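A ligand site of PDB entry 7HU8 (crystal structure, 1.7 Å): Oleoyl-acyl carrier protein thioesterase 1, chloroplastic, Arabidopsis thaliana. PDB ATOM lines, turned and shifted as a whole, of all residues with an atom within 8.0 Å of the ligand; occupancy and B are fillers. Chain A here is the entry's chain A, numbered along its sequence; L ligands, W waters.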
ATOM      1  N   ALA A  45       7.355 -27.834  19.999  1.00  0.00           N
ATOM      2  CA  ALA A  45       7.125 -28.626  18.779  1.00  0.00           C
ATOM      3  C   ALA A  45       5.881 -29.524  18.927  1.00  0.00           C
ATOM      4  O   ALA A  45       5.029 -29.563  18.022  1.00  0.00           O
ATOM      5  CB  ALA A  45       8.348 -29.475  18.472  1.00  0.00           C
ATOM      6  N   GLN A  46       5.745 -30.200  20.089  1.00  0.00           N
ATOM      7  CA  GLN A  46       4.594 -31.062  20.328  1.00  0.00           C
ATOM      8  C   GLN A  46       3.299 -30.256  20.285  1.00  0.00           C
ATOM      9  O   GLN A  46       2.327 -30.658  19.640  1.00  0.00           O
ATOM     10  CB  GLN A  46       4.729 -31.778  21.693  1.00  0.00           C
ATOM     11  CG  GLN A  46       3.757 -32.957  21.887  1.00  0.00           C
ATOM     12  CD  GLN A  46       2.317 -32.580  22.215  1.00  0.00           C
ATOM     13  OE1 GLN A  46       2.022 -31.794  23.120  1.00  0.00           O
ATOM     14  NE2 GLN A  46       1.388 -33.137  21.456  1.00  0.00           N
ATOM     15  N   SER A  47       3.280 -29.107  20.970  1.00  0.00           N
ATOM     16  CA  SER A  47       2.095 -28.269  21.084  1.00  0.00           C
ATOM     17  C   SER A  47       1.528 -27.834  19.737  1.00  0.00           C
ATOM     18  O   SER A  47       0.321 -27.690  19.620  1.00  0.00           O
ATOM     19  CB  SER A  47       2.383 -27.056  21.970  1.00  0.00           C
ATOM     20  OG  SER A  47       3.109 -26.072  21.259  1.00  0.00           O
ATOM     21  N   VAL A  48       2.391 -27.611  18.727  1.00  0.00           N
ATOM     22  CA  VAL A  48       1.894 -27.172  17.420  1.00  0.00           C
ATOM     23  C   VAL A  48       1.929 -28.261  16.325  1.00  0.00           C
ATOM     24  O   VAL A  48       1.536 -27.977  15.176  1.00  0.00           O
ATOM     25  CB  VAL A  48       2.522 -25.833  16.961  1.00  0.00           C
ATOM     26  CG1 VAL A  48       1.965 -24.678  17.806  1.00  0.00           C
ATOM     27  CG2 VAL A  48       4.044 -25.865  17.039  1.00  0.00           C
ATOM     28  N   GLY A  49       2.213 -29.505  16.689  1.00  0.00           N
ATOM     29  CA  GLY A  49       2.099 -30.631  15.778  1.00  0.00           C
ATOM     30  C   GLY A  49       3.336 -31.080  15.028  1.00  0.00           C
ATOM     31  O   GLY A  49       3.237 -31.934  14.133  1.00  0.00           O
ATOM     32  N   PHE A  50       4.511 -30.544  15.378  1.00  0.00           N
ATOM     33  CA  PHE A  50       5.770 -30.967  14.738  1.00  0.00           C
ATOM     34  C   PHE A  50       6.353 -32.217  15.425  1.00  0.00           C
ATOM     35  O   PHE A  50       5.870 -32.597  16.508  1.00  0.00           O
ATOM     36  CB  PHE A  50       6.760 -29.802  14.699  1.00  0.00           C
ATOM     37  CG  PHE A  50       6.257 -28.712  13.797  1.00  0.00           C
ATOM     38  CD1 PHE A  50       6.060 -28.936  12.452  1.00  0.00           C
ATOM     39  CD2 PHE A  50       5.855 -27.497  14.319  1.00  0.00           C
ATOM     40  CE1 PHE A  50       5.534 -27.943  11.634  1.00  0.00           C
ATOM     41  CE2 PHE A  50       5.330 -26.505  13.500  1.00  0.00           C
ATOM     42  CZ  PHE A  50       5.186 -26.737  12.158  1.00  0.00           C
ATOM     43  N   SER A  51       7.390 -32.870  14.824  1.00  0.00           N
ATOM     44  CA  SER A  51       7.961 -34.066  15.447  1.00  0.00           C
ATOM     45  C   SER A  51       8.584 -33.751  16.804  1.00  0.00           C
ATOM     46  O   SER A  51       9.018 -32.619  17.071  1.00  0.00           O
ATOM     47  CB  SER A  51       8.964 -34.783  14.545  1.00  0.00           C
ATOM     48  OG  SER A  51      10.191 -34.086  14.513  1.00  0.00           O
ATOM     49  N   ALA A  56      12.253 -31.702  15.024  1.00  0.00           N
ATOM     50  CA  ALA A  56      11.188 -30.715  14.809  1.00  0.00           C
ATOM     51  C   ALA A  56      10.723 -30.627  13.341  1.00  0.00           C
ATOM     52  O   ALA A  56      10.616 -29.543  12.789  1.00  0.00           O
ATOM     53  CB  ALA A  56      11.632 -29.365  15.324  1.00  0.00           C
ATOM     54  N   THR A  57      10.516 -31.796  12.724  1.00  0.00           N
ATOM     55  CA  THR A  57      10.129 -31.913  11.321  1.00  0.00           C
ATOM     56  C   THR A  57       8.656 -31.649  11.060  1.00  0.00           C
ATOM     57  O   THR A  57       7.812 -31.813  11.949  1.00  0.00           O
ATOM     58  CB  THR A  57      10.469 -33.337  10.807  1.00  0.00           C
ATOM     59  OG1 THR A  57       9.631 -34.299  11.467  1.00  0.00           O
ATOM     60  CG2 THR A  57      11.935 -33.694  10.992  1.00  0.00           C
ATOM     61  N   THR A  58       8.372 -31.228   9.818  1.00  0.00           N
ATOM     62  CA  THR A  58       7.047 -31.050   9.256  1.00  0.00           C
ATOM     63  C   THR A  58       6.736 -32.347   8.455  1.00  0.00           C
ATOM     64  O   THR A  58       7.636 -33.175   8.211  1.00  0.00           O
ATOM     65  CB  THR A  58       6.998 -29.817   8.308  1.00  0.00           C
ATOM     66  OG1 THR A  58       7.779 -30.058   7.124  1.00  0.00           O
ATOM     67  CG2 THR A  58       7.468 -28.515   8.968  1.00  0.00           C
ATOM     68  N   THR A  59       5.482 -32.502   8.005  1.00  0.00           N
ATOM     69  CA  THR A  59       5.077 -33.629   7.188  1.00  0.00           C
ATOM     70  C   THR A  59       5.864 -33.624   5.847  1.00  0.00           C
ATOM     71  O   THR A  59       6.226 -34.702   5.346  1.00  0.00           O
ATOM     72  CB  THR A  59       3.558 -33.563   6.920  1.00  0.00           C
ATOM     73  OG1 THR A  59       3.274 -32.293   6.318  1.00  0.00           O
ATOM     74  CG2 THR A  59       2.709 -33.705   8.197  1.00  0.00           C
ATOM     75  N   THR A  60       6.111 -32.416   5.264  1.00  0.00           N
ATOM     76  CA  THR A  60       6.846 -32.316   3.986  1.00  0.00           C
ATOM     77  C   THR A  60       8.304 -32.751   4.149  1.00  0.00           C
ATOM     78  O   THR A  60       8.853 -33.437   3.257  1.00  0.00           O
ATOM     79  CB  THR A  60       6.696 -30.903   3.393  1.00  0.00           C
ATOM     80  OG1 THR A  60       5.311 -30.645   3.215  1.00  0.00           O
ATOM     81  CG2 THR A  60       7.381 -30.773   2.041  1.00  0.00           C
ATOM     82  N   MET A  61       8.923 -32.361   5.265  1.00  0.00           N
ATOM     83  CA  MET A  61      10.307 -32.706   5.582  1.00  0.00           C
ATOM     84  C   MET A  61      10.451 -34.213   5.773  1.00  0.00           C
ATOM     85  O   MET A  61      11.412 -34.786   5.278  1.00  0.00           O
ATOM     86  CB  MET A  61      10.786 -31.975   6.835  1.00  0.00           C
ATOM     87  CG  MET A  61      10.990 -30.491   6.634  1.00  0.00           C
ATOM     88  SD  MET A  61      11.498 -29.671   8.168  1.00  0.00           S
ATOM     89  CE  MET A  61      13.117 -30.347   8.352  1.00  0.00           C
ATOM     90  N   ARG A  62       9.486 -34.863   6.450  1.00  0.00           N
ATOM     91  CA  ARG A  62       9.545 -36.317   6.657  1.00  0.00           C
ATOM     92  C   ARG A  62       9.452 -37.098   5.351  1.00  0.00           C
ATOM     93  O   ARG A  62      10.155 -38.090   5.157  1.00  0.00           O
ATOM     94  CB  ARG A  62       8.497 -36.790   7.671  1.00  0.00           C
ATOM     95  CG  ARG A  62       8.793 -36.227   9.025  1.00  0.00           C
ATOM     96  CD  ARG A  62       8.029 -36.927  10.128  1.00  0.00           C
ATOM     97  NE  ARG A  62       6.586 -36.656  10.106  1.00  0.00           N
ATOM     98  CZ  ARG A  62       6.010 -35.599  10.641  1.00  0.00           C
ATOM     99  NH1 ARG A  62       4.684 -35.473  10.623  1.00  0.00           N
ATOM    100  NH2 ARG A  62       6.740 -34.634  11.185  1.00  0.00           N
ATOM    101  N   ASP A 139       8.014 -24.074   0.399  1.00  0.00           N
ATOM    102  CA  ASP A 139       6.962 -24.936   0.953  1.00  0.00           C
ATOM    103  C   ASP A 139       7.150 -25.188   2.451  1.00  0.00           C
ATOM    104  O   ASP A 139       6.178 -25.116   3.201  1.00  0.00           O
ATOM    105  CB  ASP A 139       6.933 -26.284   0.206  1.00  0.00           C
ATOM    106  CG  ASP A 139       6.320 -26.238  -1.169  1.00  0.00           C
ATOM    107  OD1 ASP A 139       5.687 -25.203  -1.497  1.00  0.00           O
ATOM    108  OD2 ASP A 139       6.470 -27.235  -1.922  1.00  0.00           O
ATOM    109  N   VAL A 140       8.396 -25.489   2.876  1.00  0.00           N
ATOM    110  CA  VAL A 140       8.720 -25.757   4.268  1.00  0.00           C
ATOM    111  C   VAL A 140       8.615 -24.466   5.073  1.00  0.00           C
ATOM    112  O   VAL A 140       7.968 -24.466   6.116  1.00  0.00           O
ATOM    113  CB  VAL A 140      10.104 -26.457   4.426  1.00  0.00           C
ATOM    114  CG1 VAL A 140      10.499 -26.596   5.892  1.00  0.00           C
ATOM    115  CG2 VAL A 140      10.085 -27.811   3.742  1.00  0.00           C
ATOM    116  N   ASP A 142       6.703 -21.833   4.605  1.00  0.00           N
ATOM    117  CA  ASP A 142       5.280 -21.531   4.783  1.00  0.00           C
ATOM    118  C   ASP A 142       4.602 -22.409   5.837  1.00  0.00           C
ATOM    119  O   ASP A 142       3.619 -21.973   6.449  1.00  0.00           O
ATOM    120  CB  ASP A 142       4.542 -21.609   3.429  1.00  0.00           C
ATOM    121  CG  ASP A 142       4.973 -20.561   2.403  1.00  0.00           C
ATOM    122  OD1 ASP A 142       5.864 -19.720   2.736  1.00  0.00           O
ATOM    123  OD2 ASP A 142       4.453 -20.600   1.260  1.00  0.00           O
ATOM    124  N   GLU A 143       5.101 -23.633   6.045  1.00  0.00           N
ATOM    125  CA  GLU A 143       4.537 -24.529   7.054  1.00  0.00           C
ATOM    126  C   GLU A 143       4.822 -24.047   8.482  1.00  0.00           C
ATOM    127  O   GLU A 143       3.987 -24.229   9.349  1.00  0.00           O
ATOM    128  CB  GLU A 143       5.070 -25.968   6.893  1.00  0.00           C
ATOM    129  CG  GLU A 143       4.513 -26.752   5.718  1.00  0.00           C
ATOM    130  CD  GLU A 143       5.185 -28.097   5.567  1.00  0.00           C
ATOM    131  OE1 GLU A 143       6.430 -28.142   5.674  1.00  0.00           O
ATOM    132  OE2 GLU A 143       4.477 -29.104   5.381  1.00  0.00           O
ATOM    133  N   TYR A 144       5.965 -23.384   8.688  1.00  0.00           N
ATOM    134  CA  TYR A 144       6.494 -22.923   9.980  1.00  0.00           C
ATOM    135  C   TYR A 144       6.186 -21.458  10.337  1.00  0.00           C
ATOM    136  O   TYR A 144       6.033 -21.121  11.506  1.00  0.00           O
ATOM    137  CB  TYR A 144       8.030 -23.068   9.925  1.00  0.00           C
ATOM    138  CG  TYR A 144       8.758 -23.511  11.184  1.00  0.00           C
ATOM    139  CD1 TYR A 144       8.448 -22.970  12.419  1.00  0.00           C
ATOM    140  CD2 TYR A 144       9.849 -24.362  11.095  1.00  0.00           C
ATOM    141  CE1 TYR A 144       9.157 -23.339  13.568  1.00  0.00           C
ATOM    142  CE2 TYR A 144      10.572 -24.729  12.235  1.00  0.00           C
ATOM    143  CZ  TYR A 144      10.212 -24.229  13.469  1.00  0.00           C
ATOM    144  OH  TYR A 144      10.936 -24.606  14.577  1.00  0.00           O
ATOM    145  N   VAL A 146       3.740 -19.425  10.350  1.00  0.00           N
ATOM    146  CA  VAL A 146       2.552 -19.118  11.142  1.00  0.00           C
ATOM    147  C   VAL A 146       2.758 -19.399  12.657  1.00  0.00           C
ATOM    148  O   VAL A 146       1.939 -18.994  13.472  1.00  0.00           O
ATOM    149  CB  VAL A 146       1.287 -19.846  10.611  1.00  0.00           C
ATOM    150  CG1 VAL A 146       0.958 -19.397   9.191  1.00  0.00           C
ATOM    151  CG2 VAL A 146       1.469 -21.348  10.665  1.00  0.00           C
ATOM    152  N   PHE A 147       3.798 -20.153  13.011  1.00  0.00           N
ATOM    153  CA  PHE A 147       4.101 -20.460  14.412  1.00  0.00           C
ATOM    154  C   PHE A 147       5.190 -19.508  14.998  1.00  0.00           C
ATOM    155  O   PHE A 147       5.515 -19.595  16.175  1.00  0.00           O
ATOM    156  CB  PHE A 147       4.484 -21.948  14.555  1.00  0.00           C
ATOM    157  CG  PHE A 147       3.426 -22.863  13.994  1.00  0.00           C
ATOM    158  CD1 PHE A 147       2.170 -22.952  14.590  1.00  0.00           C
ATOM    159  CD2 PHE A 147       3.612 -23.546  12.808  1.00  0.00           C
ATOM    160  CE1 PHE A 147       1.171 -23.740  14.045  1.00  0.00           C
ATOM    161  CE2 PHE A 147       2.622 -24.356  12.271  1.00  0.00           C
ATOM    162  CZ  PHE A 147       1.391 -24.436  12.885  1.00  0.00           C
HETATM  163  N1  LIG L   1       3.306 -29.094   8.505  1.00  0.00           N
HETATM  164  C1  LIG L   1       0.803 -27.345  10.522  1.00  0.00           C
HETATM  165  C2  LIG L   1       0.083 -27.998  11.700  1.00  0.00           C
HETATM  166  C3  LIG L   1       1.031 -28.868  12.505  1.00  0.00           C
HETATM  167  C4  LIG L   1       1.699 -29.929  11.630  1.00  0.00           C
HETATM  168  C5  LIG L   1       3.161 -29.890   9.570  1.00  0.00           C
HETATM  169  C6  LIG L   1       2.292 -28.054   8.459  1.00  0.00           C
HETATM  170  C7  LIG L   1       1.368 -28.435   9.614  1.00  0.00           C
HETATM  171  N2  LIG L   1       2.222 -29.316  10.414  1.00  0.00           N
HETATM  172  O1  LIG L   1       3.758 -30.932   9.794  1.00  0.00           O
HETATM  173  O   HOH W   1       4.269 -32.768  11.595  1.00  0.00           O
HETATM  174  O   HOH W   2       1.349 -24.486   8.676  1.00  0.00           O
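Merely in contact with the ligand: Val 48, Thr 58, Gly 49, Phe 50 and Phe 147. Hydrophobic or aromatic side chains within 4 Å of the ligand: Phe 50 and Phe 147. Along chain A the residues within 4 Å of the ligand span positions 48 to 147.
O of Thr 58 sits close to NH2 of Arg 62 (3.4 Å). OE2 of Glu 143 is in hydrogen-bond range of OG1 of Thr 60, 2.8 Å away. The side-chain hydroxyl (OG1) of Thr 58 is in hydrogen-bond range of the side-chain carboxylate (OE1) of Glu 143, 2.8 Å away. N of Met 61 lies within hydrogen-bond range of OG1 of Thr 58. The backbone NH of Phe 50 sits at hydrogen-bond distance from the backbone carbonyl oxygen of Ala 45 (2.9 Å). The backbone NH of Thr 60 sits close to the side-chain hydroxyl of Thr 58 (3.4 Å).
N of Thr 59 lies within hydrogen-bond range of O1 of the ligand (2.9 Å). The side-chain carboxylate of Glu 143 is in hydrogen-bond range of a nitrogen (N1) of the ligand, 3.3 Å away.
Water W1 lies within hydrogen-bond range of an oxygen (O1) of the ligand (2.6 Å), the backbone carbonyl oxygen (O) of Gly 49 (2.9 Å) and the guanidinium group (NH1) of Arg 62 (2.9 Å).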
